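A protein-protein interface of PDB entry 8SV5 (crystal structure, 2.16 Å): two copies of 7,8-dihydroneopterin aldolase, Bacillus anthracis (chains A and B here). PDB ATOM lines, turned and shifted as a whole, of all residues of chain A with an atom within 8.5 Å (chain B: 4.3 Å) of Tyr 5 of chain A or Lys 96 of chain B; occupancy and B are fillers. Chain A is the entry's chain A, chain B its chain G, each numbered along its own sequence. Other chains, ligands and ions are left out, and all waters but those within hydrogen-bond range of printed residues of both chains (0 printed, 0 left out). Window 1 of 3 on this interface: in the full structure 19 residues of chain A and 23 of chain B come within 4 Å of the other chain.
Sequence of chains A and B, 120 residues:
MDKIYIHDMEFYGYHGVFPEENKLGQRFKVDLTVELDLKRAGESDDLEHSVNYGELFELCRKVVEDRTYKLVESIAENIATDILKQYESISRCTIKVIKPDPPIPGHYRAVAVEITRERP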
ATOM      1  N   MET A   1     -17.767  -2.414  21.353  1.00  0.00           N
ATOM      2  CA  MET A   1     -17.610  -2.979  19.981  1.00  0.00           C
ATOM      3  C   MET A   1     -18.086  -1.966  18.945  1.00  0.00           C
ATOM      4  O   MET A   1     -18.328  -0.802  19.268  1.00  0.00           O
ATOM      5  CB  MET A   1     -18.408  -4.277  19.828  1.00  0.00           C
ATOM      6  CG  MET A   1     -18.802  -4.949  21.137  1.00  0.00           C
ATOM      7  SD  MET A   1     -19.866  -6.384  20.876  1.00  0.00           S
ATOM      8  CE  MET A   1     -18.680  -7.585  20.274  1.00  0.00           C
ATOM      9  N   ASP A   2     -18.222  -2.413  17.699  1.00  0.00           N
ATOM     10  CA  ASP A   2     -18.735  -1.548  16.649  1.00  0.00           C
ATOM     11  C   ASP A   2     -20.180  -1.162  16.958  1.00  0.00           C
ATOM     12  O   ASP A   2     -20.850  -1.763  17.799  1.00  0.00           O
ATOM     13  CB  ASP A   2     -18.651  -2.250  15.299  1.00  0.00           C
ATOM     14  CG  ASP A   2     -17.263  -2.785  15.012  1.00  0.00           C
ATOM     15  OD1 ASP A   2     -16.282  -2.182  15.499  1.00  0.00           O
ATOM     16  OD2 ASP A   2     -17.150  -3.810  14.307  1.00  0.00           O
ATOM     17  N   LYS A   3     -20.663  -0.139  16.255  1.00  0.00           N
ATOM     18  CA  LYS A   3     -21.953   0.451  16.563  1.00  0.00           C
ATOM     19  C   LYS A   3     -22.689   0.821  15.286  1.00  0.00           C
ATOM     20  O   LYS A   3     -22.079   1.167  14.271  1.00  0.00           O
ATOM     21  CB  LYS A   3     -21.786   1.713  17.421  1.00  0.00           C
ATOM     22  CG  LYS A   3     -21.126   1.460  18.764  1.00  0.00           C
ATOM     23  CD  LYS A   3     -21.132   2.707  19.632  1.00  0.00           C
ATOM     24  CE  LYS A   3     -20.244   2.533  20.854  1.00  0.00           C
ATOM     25  NZ  LYS A   3     -20.849   3.137  22.075  1.00  0.00           N
ATOM     26  N   ILE A   4     -24.016   0.733  15.351  1.00  0.00           N
ATOM     27  CA  ILE A   4     -24.911   1.283  14.342  1.00  0.00           C
ATOM     28  C   ILE A   4     -25.781   2.322  15.033  1.00  0.00           C
ATOM     29  O   ILE A   4     -26.406   2.030  16.060  1.00  0.00           O
ATOM     30  CB  ILE A   4     -25.778   0.192  13.689  1.00  0.00           C
ATOM     31  CG1 ILE A   4     -24.931  -0.652  12.736  1.00  0.00           C
ATOM     32  CG2 ILE A   4     -26.954   0.812  12.932  1.00  0.00           C
ATOM     33  CD1 ILE A   4     -25.568  -1.963  12.350  1.00  0.00           C
ATOM     34  N   TYR A   5     -25.812   3.531  14.479  1.00  0.00           N
ATOM     35  CA  TYR A   5     -26.602   4.619  15.022  1.00  0.00           C
ATOM     36  C   TYR A   5     -27.778   4.920  14.101  1.00  0.00           C
ATOM     37  O   TYR A   5     -27.682   4.791  12.877  1.00  0.00           O
ATOM     38  CB  TYR A   5     -25.781   5.910  15.139  1.00  0.00           C
ATOM     39  CG  TYR A   5     -24.632   5.877  16.120  1.00  0.00           C
ATOM     40  CD1 TYR A   5     -24.842   6.087  17.477  1.00  0.00           C
ATOM     41  CD2 TYR A   5     -23.331   5.672  15.681  1.00  0.00           C
ATOM     42  CE1 TYR A   5     -23.787   6.072  18.372  1.00  0.00           C
ATOM     43  CE2 TYR A   5     -22.272   5.656  16.568  1.00  0.00           C
ATOM     44  CZ  TYR A   5     -22.506   5.857  17.911  1.00  0.00           C
ATOM     45  OH  TYR A   5     -21.456   5.843  18.798  1.00  0.00           O
ATOM     46  N   ILE A   6     -28.889   5.326  14.705  1.00  0.00           N
ATOM     47  CA  ILE A   6     -29.961   6.029  14.011  1.00  0.00           C
ATOM     48  C   ILE A   6     -30.203   7.300  14.811  1.00  0.00           C
ATOM     49  O   ILE A   6     -30.660   7.237  15.960  1.00  0.00           O
ATOM     50  CB  ILE A   6     -31.242   5.196  13.890  1.00  0.00           C
ATOM     51  CG1 ILE A   6     -30.921   3.820  13.295  1.00  0.00           C
ATOM     52  CG2 ILE A   6     -32.270   5.946  13.038  1.00  0.00           C
ATOM     53  CD1 ILE A   6     -32.135   3.050  12.816  1.00  0.00           C
ATOM     54  N   HIS A   7     -29.884   8.449  14.220  1.00  0.00           N
ATOM     55  CA  HIS A   7     -29.904   9.714  14.935  1.00  0.00           C
ATOM     56  C   HIS A   7     -31.245  10.412  14.758  1.00  0.00           C
ATOM     57  O   HIS A   7     -31.707  10.608  13.630  1.00  0.00           O
ATOM     58  CB  HIS A   7     -28.805  10.643  14.414  1.00  0.00           C
ATOM     59  CG  HIS A   7     -27.417  10.161  14.694  1.00  0.00           C
ATOM     60  ND1 HIS A   7     -26.984   9.823  15.958  1.00  0.00           N
ATOM     61  CD2 HIS A   7     -26.360   9.971  13.870  1.00  0.00           C
ATOM     62  CE1 HIS A   7     -25.721   9.440  15.899  1.00  0.00           C
ATOM     63  NE2 HIS A   7     -25.319   9.520  14.644  1.00  0.00           N
ATOM     64  N   ASP A   8     -31.859  10.789  15.877  1.00  0.00           N
ATOM     65  CA  ASP A   8     -32.923  11.790  15.886  1.00  0.00           C
ATOM     66  C   ASP A   8     -34.138  11.355  15.074  1.00  0.00           C
ATOM     67  O   ASP A   8     -34.712  12.137  14.313  1.00  0.00           O
ATOM     68  CB  ASP A   8     -32.395  13.144  15.396  1.00  0.00           C
ATOM     69  CG  ASP A   8     -33.043  14.317  16.105  1.00  0.00           C
ATOM     70  OD1 ASP A   8     -32.710  14.554  17.285  1.00  0.00           O
ATOM     71  OD2 ASP A   8     -33.885  15.002  15.486  1.00  0.00           O
ATOM     72  N   MET A   9     -34.540  10.098  15.231  1.00  0.00           N
ATOM     73  CA  MET A   9     -35.818   9.670  14.681  1.00  0.00           C
ATOM     74  C   MET A   9     -36.921  10.539  15.269  1.00  0.00           C
ATOM     75  O   MET A   9     -36.901  10.862  16.457  1.00  0.00           O
ATOM     76  CB  MET A   9     -36.075   8.213  15.052  1.00  0.00           C
ATOM     77  CG  MET A   9     -35.267   7.214  14.252  1.00  0.00           C
ATOM     78  SD  MET A   9     -35.496   5.532  14.856  1.00  0.00           S
ATOM     79  CE  MET A   9     -34.239   5.465  16.125  1.00  0.00           C
ATOM     80  N   VAL A  30     -36.337   9.656  19.058  1.00  0.00           N
ATOM     81  CA  VAL A  30     -35.571   8.522  19.559  1.00  0.00           C
ATOM     82  C   VAL A  30     -34.168   8.564  18.966  1.00  0.00           C
ATOM     83  O   VAL A  30     -34.001   8.789  17.760  1.00  0.00           O
ATOM     84  CB  VAL A  30     -36.247   7.175  19.243  1.00  0.00           C
ATOM     85  CG1 VAL A  30     -35.389   6.012  19.740  1.00  0.00           C
ATOM     86  CG2 VAL A  30     -37.632   7.110  19.869  1.00  0.00           C
ATOM     87  N   ASP A  31     -33.171   8.349  19.813  1.00  0.00           N
ATOM     88  CA  ASP A  31     -31.803   8.090  19.395  1.00  0.00           C
ATOM     89  C   ASP A  31     -31.498   6.630  19.698  1.00  0.00           C
ATOM     90  O   ASP A  31     -31.716   6.172  20.826  1.00  0.00           O
ATOM     91  CB  ASP A  31     -30.827   8.989  20.152  1.00  0.00           C
ATOM     92  CG  ASP A  31     -30.500  10.259  19.392  1.00  0.00           C
ATOM     93  OD1 ASP A  31     -30.370  10.194  18.151  1.00  0.00           O
ATOM     94  OD2 ASP A  31     -30.374  11.324  20.036  1.00  0.00           O
ATOM     95  N   LEU A  32     -31.009   5.901  18.699  1.00  0.00           N
ATOM     96  CA  LEU A  32     -30.779   4.467  18.819  1.00  0.00           C
ATOM     97  C   LEU A  32     -29.310   4.158  18.576  1.00  0.00           C
ATOM     98  O   LEU A  32     -28.723   4.631  17.598  1.00  0.00           O
ATOM     99  CB  LEU A  32     -31.643   3.684  17.825  1.00  0.00           C
ATOM    100  CG  LEU A  32     -31.505   2.159  17.866  1.00  0.00           C
ATOM    101  CD1 LEU A  32     -31.701   1.636  19.276  1.00  0.00           C
ATOM    102  CD2 LEU A  32     -32.498   1.493  16.931  1.00  0.00           C
ATOM    103  N   THR A  33     -28.725   3.361  19.468  1.00  0.00           N
ATOM    104  CA  THR A  33     -27.382   2.828  19.296  1.00  0.00           C
ATOM    105  C   THR A  33     -27.417   1.349  19.650  1.00  0.00           C
ATOM    106  O   THR A  33     -27.955   0.971  20.695  1.00  0.00           O
ATOM    107  CB  THR A  33     -26.375   3.553  20.194  1.00  0.00           C
ATOM    108  OG1 THR A  33     -26.424   4.962  19.938  1.00  0.00           O
ATOM    109  CG2 THR A  33     -24.962   3.047  19.934  1.00  0.00           C
ATOM    110  N   VAL A  34     -26.858   0.518  18.775  1.00  0.00           N
ATOM    111  CA  VAL A  34     -26.774  -0.921  18.991  1.00  0.00           C
ATOM    112  C   VAL A  34     -25.343  -1.356  18.713  1.00  0.00           C
ATOM    113  O   VAL A  34     -24.685  -0.814  17.818  1.00  0.00           O
ATOM    114  CB  VAL A  34     -27.771  -1.689  18.099  1.00  0.00           C
ATOM    115  CG1 VAL A  34     -29.199  -1.264  18.417  1.00  0.00           C
ATOM    116  CG2 VAL A  34     -27.460  -1.468  16.625  1.00  0.00           C
ATOM    117  N   GLU A  35     -24.861  -2.327  19.484  1.00  0.00           N
ATOM    118  CA  GLU A  35     -23.481  -2.785  19.393  1.00  0.00           C
ATOM    119  C   GLU A  35     -23.432  -4.237  18.937  1.00  0.00           C
ATOM    120  O   GLU A  35     -24.252  -5.062  19.349  1.00  0.00           O
ATOM    121  CB  GLU A  35     -22.761  -2.627  20.735  1.00  0.00           C
ATOM    122  CG  GLU A  35     -23.234  -1.428  21.543  1.00  0.00           C
ATOM    123  CD  GLU A  35     -22.243  -1.014  22.615  1.00  0.00           C
ATOM    124  OE1 GLU A  35     -21.158  -1.628  22.696  1.00  0.00           O
ATOM    125  OE2 GLU A  35     -22.550  -0.072  23.375  1.00  0.00           O
ATOM    126  N   LEU A  36     -22.455  -4.531  18.085  1.00  0.00           N
ATOM    127  CA  LEU A  36     -22.269  -5.841  17.476  1.00  0.00           C
ATOM    128  C   LEU A  36     -20.946  -5.779  16.726  1.00  0.00           C
ATOM    129  O   LEU A  36     -20.375  -4.702  16.538  1.00  0.00           O
ATOM    130  CB  LEU A  36     -23.420  -6.187  16.529  1.00  0.00           C
ATOM    131  CG  LEU A  36     -23.531  -5.374  15.234  1.00  0.00           C
ATOM    132  CD1 LEU A  36     -24.508  -6.032  14.270  1.00  0.00           C
ATOM    133  CD2 LEU A  36     -23.950  -3.934  15.504  1.00  0.00           C
ATOM    134  N   LEU A  38     -19.002  -5.699  13.437  1.00  0.00           N
ATOM    135  CA  LEU A  38     -19.233  -5.346  12.048  1.00  0.00           C
ATOM    136  C   LEU A  38     -18.052  -5.688  11.151  1.00  0.00           C
ATOM    137  O   LEU A  38     -18.130  -5.465   9.938  1.00  0.00           O
ATOM    138  CB  LEU A  38     -19.556  -3.853  11.934  1.00  0.00           C
ATOM    139  CG  LEU A  38     -20.885  -3.430  12.563  1.00  0.00           C
ATOM    140  CD1 LEU A  38     -21.080  -1.929  12.430  1.00  0.00           C
ATOM    141  CD2 LEU A  38     -22.057  -4.174  11.939  1.00  0.00           C
ATOM    142  N   TYR A  53     -30.436  -1.621   9.015  1.00  0.00           N
ATOM    143  CA  TYR A  53     -30.826  -0.477   9.836  1.00  0.00           C
ATOM    144  C   TYR A  53     -32.257  -0.028   9.555  1.00  0.00           C
ATOM    145  O   TYR A  53     -32.873   0.608  10.417  1.00  0.00           O
ATOM    146  CB  TYR A  53     -29.819   0.673   9.686  1.00  0.00           C
ATOM    147  CG  TYR A  53     -29.585   1.183   8.276  1.00  0.00           C
ATOM    148  CD1 TYR A  53     -30.644   1.526   7.454  1.00  0.00           C
ATOM    149  CD2 TYR A  53     -28.299   1.345   7.778  1.00  0.00           C
ATOM    150  CE1 TYR A  53     -30.437   1.994   6.175  1.00  0.00           C
ATOM    151  CE2 TYR A  53     -28.083   1.823   6.496  1.00  0.00           C
ATOM    152  CZ  TYR A  53     -29.163   2.145   5.702  1.00  0.00           C
ATOM    153  OH  TYR A  53     -28.985   2.620   4.426  1.00  0.00           O
ATOM    154  N   LEU A  56     -34.476  -1.684  11.942  1.00  0.00           N
ATOM    155  CA  LEU A  56     -34.349  -1.087  13.267  1.00  0.00           C
ATOM    156  C   LEU A  56     -35.202   0.170  13.387  1.00  0.00           C
ATOM    157  O   LEU A  56     -35.776   0.436  14.450  1.00  0.00           O
ATOM    158  CB  LEU A  56     -32.883  -0.778  13.567  1.00  0.00           C
ATOM    159  CG  LEU A  56     -31.986  -1.992  13.816  1.00  0.00           C
ATOM    160  CD1 LEU A  56     -30.536  -1.566  13.984  1.00  0.00           C
ATOM    161  CD2 LEU A  56     -32.454  -2.781  15.035  1.00  0.00           C
ATOM    162  N   THR A  94     -28.508   0.981  23.420  1.00  0.00           N
ATOM    163  CA  THR A  94     -28.785   2.162  24.227  1.00  0.00           C
ATOM    164  C   THR A  94     -29.914   2.920  23.547  1.00  0.00           C
ATOM    165  O   THR A  94     -29.769   3.355  22.399  1.00  0.00           O
ATOM    166  CB  THR A  94     -27.539   3.045  24.330  1.00  0.00           C
ATOM    167  OG1 THR A  94     -26.390   2.229  24.595  1.00  0.00           O
ATOM    168  CG2 THR A  94     -27.690   4.077  25.444  1.00  0.00           C
ATOM    169  N   LYS B  29     -21.203  11.055   4.622  1.00  0.00           N
ATOM    170  CA  LYS B  29     -20.405  11.839   5.552  1.00  0.00           C
ATOM    171  C   LYS B  29     -19.514  10.911   6.363  1.00  0.00           C
ATOM    172  O   LYS B  29     -19.837   9.738   6.572  1.00  0.00           O
ATOM    173  CB  LYS B  29     -21.291  12.678   6.483  1.00  0.00           C
ATOM    174  CG  LYS B  29     -21.559  14.090   5.956  1.00  0.00           C
ATOM    175  CD  LYS B  29     -23.028  14.490   6.071  1.00  0.00           C
ATOM    176  CE  LYS B  29     -23.238  15.564   7.128  1.00  0.00           C
ATOM    177  NZ  LYS B  29     -24.457  16.379   6.869  1.00  0.00           N
ATOM    178  N   VAL B  30     -18.380  11.447   6.810  1.00  0.00           N
ATOM    179  CA  VAL B  30     -17.397  10.681   7.567  1.00  0.00           C
ATOM    180  C   VAL B  30     -16.863  11.545   8.701  1.00  0.00           C
ATOM    181  O   VAL B  30     -16.495  12.705   8.486  1.00  0.00           O
ATOM    182  CB  VAL B  30     -16.240  10.197   6.667  1.00  0.00           C
ATOM    183  CG1 VAL B  30     -15.183   9.469   7.489  1.00  0.00           C
ATOM    184  CG2 VAL B  30     -16.765   9.294   5.559  1.00  0.00           C
ATOM    185  N   ASP B  31     -16.826  10.982   9.905  1.00  0.00           N
ATOM    186  CA  ASP B  31     -16.133  11.570  11.044  1.00  0.00           C
ATOM    187  C   ASP B  31     -14.916  10.701  11.327  1.00  0.00           C
ATOM    188  O   ASP B  31     -15.049   9.488  11.530  1.00  0.00           O
ATOM    189  CB  ASP B  31     -17.034  11.618  12.276  1.00  0.00           C
ATOM    190  CG  ASP B  31     -18.101  12.689  12.178  1.00  0.00           C
ATOM    191  OD1 ASP B  31     -17.858  13.719  11.515  1.00  0.00           O
ATOM    192  OD2 ASP B  31     -19.189  12.499  12.766  1.00  0.00           O
ATOM    193  N   THR B  94     -10.942   5.637  14.951  1.00  0.00           N
ATOM    194  CA  THR B  94     -12.387   5.453  15.002  1.00  0.00           C
ATOM    195  C   THR B  94     -12.988   6.117  13.774  1.00  0.00           C
ATOM    196  O   THR B  94     -12.772   7.313  13.543  1.00  0.00           O
ATOM    197  CB  THR B  94     -12.965   6.064  16.281  1.00  0.00           C
ATOM    198  OG1 THR B  94     -12.283   5.525  17.421  1.00  0.00           O
ATOM    199  CG2 THR B  94     -14.457   5.769  16.395  1.00  0.00           C
ATOM    200  N   ILE B  95     -13.734   5.344  12.987  1.00  0.00           N
ATOM    201  CA  ILE B  95     -14.323   5.805  11.735  1.00  0.00           C
ATOM    202  C   ILE B  95     -15.836   5.748  11.881  1.00  0.00           C
ATOM    203  O   ILE B  95     -16.393   4.688  12.198  1.00  0.00           O
ATOM    204  CB  ILE B  95     -13.871   4.948  10.541  1.00  0.00           C
ATOM    205  CG1 ILE B  95     -12.363   4.686  10.595  1.00  0.00           C
ATOM    206  CG2 ILE B  95     -14.263   5.619   9.226  1.00  0.00           C
ATOM    207  CD1 ILE B  95     -11.518   5.927  10.485  1.00  0.00           C
ATOM    208  N   LYS B  96     -16.499   6.877  11.645  1.00  0.00           N
ATOM    209  CA  LYS B  96     -17.956   6.957  11.645  1.00  0.00           C
ATOM    210  C   LYS B  96     -18.400   7.342  10.242  1.00  0.00           C
ATOM    211  O   LYS B  96     -18.141   8.463   9.791  1.00  0.00           O
ATOM    212  CB  LYS B  96     -18.447   7.980  12.666  1.00  0.00           C
ATOM    213  CG  LYS B  96     -19.951   7.940  12.905  1.00  0.00           C
ATOM    214  CD  LYS B  96     -20.386   9.042  13.853  1.00  0.00           C
ATOM    215  CE  LYS B  96     -21.826   8.858  14.294  1.00  0.00           C
ATOM    216  NZ  LYS B  96     -22.353  10.080  14.962  1.00  0.00           N
ATOM    217  N   VAL B  97     -19.055   6.415   9.551  1.00  0.00           N
ATOM    218  CA  VAL B  97     -19.584   6.649   8.212  1.00  0.00           C
ATOM    219  C   VAL B  97     -21.076   6.914   8.346  1.00  0.00           C
ATOM    220  O   VAL B  97     -21.818   6.082   8.880  1.00  0.00           O
ATOM    221  CB  VAL B  97     -19.310   5.455   7.285  1.00  0.00           C
ATOM    222  CG1 VAL B  97     -19.941   5.684   5.920  1.00  0.00           C
ATOM    223  CG2 VAL B  97     -17.810   5.225   7.148  1.00  0.00           C
ATOM    224  N   ILE B  98     -21.514   8.070   7.856  1.00  0.00           N
ATOM    225  CA  ILE B  98     -22.873   8.556   8.055  1.00  0.00           C
ATOM    226  C   ILE B  98     -23.594   8.551   6.717  1.00  0.00           C
ATOM    227  O   ILE B  98     -23.040   8.989   5.703  1.00  0.00           O
ATOM    228  CB  ILE B  98     -22.874   9.967   8.673  1.00  0.00           C
ATOM    229  CG1 ILE B  98     -22.190   9.949  10.039  1.00  0.00           C
ATOM    230  CG2 ILE B  98     -24.300  10.500   8.799  1.00  0.00           C
ATOM    231  CD1 ILE B  98     -21.179  11.055  10.227  1.00  0.00           C
ATOM    232  N   VAL B 111     -28.508   7.799   9.553  1.00  0.00           N
ATOM    233  CA  VAL B 111     -28.059   6.505  10.049  1.00  0.00           C
ATOM    234  C   VAL B 111     -26.544   6.473   9.902  1.00  0.00           C
ATOM    235  O   VAL B 111     -25.973   7.169   9.055  1.00  0.00           O
ATOM    236  CB  VAL B 111     -28.717   5.322   9.307  1.00  0.00           C
ATOM    237  CG1 VAL B 111     -30.232   5.359   9.488  1.00  0.00           C
ATOM    238  CG2 VAL B 111     -28.352   5.336   7.829  1.00  0.00           C
ATOM    239  N   ALA B 112     -25.891   5.664  10.728  1.00  0.00           N
ATOM    240  CA  ALA B 112     -24.437   5.643  10.705  1.00  0.00           C
ATOM    241  C   ALA B 112     -23.922   4.341  11.293  1.00  0.00           C
ATOM    242  O   ALA B 112     -24.585   3.711  12.121  1.00  0.00           O
ATOM    243  CB  ALA B 112     -23.854   6.827  11.488  1.00  0.00           C
ATOM    244  N   VAL B 113     -22.731   3.953  10.843  1.00  0.00           N
ATOM    245  CA  VAL B 113     -21.965   2.864  11.432  1.00  0.00           C
ATOM    246  C   VAL B 113     -20.658   3.448  11.948  1.00  0.00           C
ATOM    247  O   VAL B 113     -20.078   4.343  11.324  1.00  0.00           O
ATOM    248  CB  VAL B 113     -21.694   1.732  10.418  1.00  0.00           C
ATOM    249  CG1 VAL B 113     -22.996   1.229   9.825  1.00  0.00           C
ATOM    250  CG2 VAL B 113     -20.757   2.201   9.313  1.00  0.00           C
ATOM    251  N   GLU B 114     -20.200   2.946  13.089  1.00  0.00           N
ATOM    252  CA  GLU B 114     -18.963   3.405  13.698  1.00  0.00           C
ATOM    253  C   GLU B 114     -18.146   2.201  14.133  1.00  0.00           C
ATOM    254  O   GLU B 114     -18.685   1.251  14.711  1.00  0.00           O
ATOM    255  CB  GLU B 114     -19.241   4.298  14.911  1.00  0.00           C
ATOM    256  CG  GLU B 114     -17.992   4.698  15.679  1.00  0.00           C
ATOM    257  CD  GLU B 114     -18.277   5.722  16.762  1.00  0.00           C
ATOM    258  OE1 GLU B 114     -18.330   6.930  16.444  1.00  0.00           O
ATOM    259  OE2 GLU B 114     -18.451   5.316  17.932  1.00  0.00           O
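Of the 12 printed residues of chain B, 5 touch a printed residue of chain A.
Hydrophobic or aromatic side chains of chain B that line the printed part of chain A: Val 111 and Val 113.
Of the 20 printed residues of chain A, 6 touch a printed residue of chain B.
Along chain A the printed residues that touch a printed residue of chain B span positions 2 to 53.
Among the printed residues, 11 pairs touch across the chains.
CA of Asp 2 of chain A touches O of Glu 114 of chain B (3.4 Å).
O of Lys 3 of chain A touches CA of Val 113 of chain B, at 3.3 Å.
Ala 112 of chain B touches Ile 4 of chain A (O to CA, 3.3 Å).
Ile 4 of chain A touches Val 113 of chain B (CG1 to CG1, 3.97 Å).
CE of Lys 96 of chain B touches CD2 of Tyr 5 of chain A (3.8 Å).
Tyr 5 of chain A touches Val 111 of chain B.
Tyr 53 of chain A touches Val 111 of chain B (CE2 to CG2, 3.8 Å).
The side-chain hydroxyl (OH) of Tyr 5 of chain A sits at hydrogen-bond distance from the side-chain carboxylate (OE2) of Glu 114 of chain B (3.2 Å).
The backbone NH of Tyr 5 of chain A lies within hydrogen-bond range of the backbone carbonyl oxygen of Ala 112 of chain B (2.7 Å).
O of Lys 3 of chain A is in hydrogen-bond range of N of Glu 114 of chain B, 2.8 Å away.
A ring nitrogen (NE2) of His 7 of chain A lies within hydrogen-bond range of the side-chain amino group of Lys 96 of chain B (3.0 Å).
Positions printed for both chains: 30, 31 and 94.
The backbone NH (N) of Ile 4 of chain A sits at hydrogen-bond distance from the backbone carbonyl oxygen (O) of Val 34 of chain A.
OE2 of Glu 35 of chain A lies within salt-bridge range of NZ of Lys 3 of chain A.
The backbone NH of Val 97 of chain B lies within hydrogen-bond range of the backbone carbonyl oxygen of Val 113 of chain B, at 2.9 Å.
OD2 of Asp 2 of chain A sits at hydrogen-bond distance from N of Leu 38 of chain A.
The backbone carbonyl oxygen (O) of Asp 2 of chain A lies within hydrogen-bond range of the backbone NH (N) of Leu 36 of chain A, 3.2 Å away.
The backbone NH (N) of Asp 31 of chain B sits at hydrogen-bond distance from the backbone carbonyl oxygen (O) of Lys 96 of chain B, at 2.8 Å.
Of the printed residues of chain B, Asp 2 of chain A touches Glu 114 (3.4 Å).
Of the printed residues of chain B, Lys 3 of chain A touches Val 113 (3.3 Å) and Glu 114 (2.8 Å).
Tyr 5 of chain A touches just these residues of chain B: Lys 96, Val 111, Ala 112 and Glu 114.
Thr 33 of chain A touches none of the printed residues of chain B.
Of chain A, only Tyr 5 and His 7 come within 4 Å of Lys 96 of chain B.
Ala 112 of chain B touches just these residues of chain A: Ile 4 and Tyr 5.
Of the printed residues of chain A, Val 113 of chain B touches Lys 3 and Ile 4.
The nearest residue of chain A that does not touch Lys 96 of chain B is Lys 3 of chain A (7.2 Å).
The nearest printed residue of chain A that does not touch Glu 114 of chain B is Leu 38 of chain A (4.6 Å).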
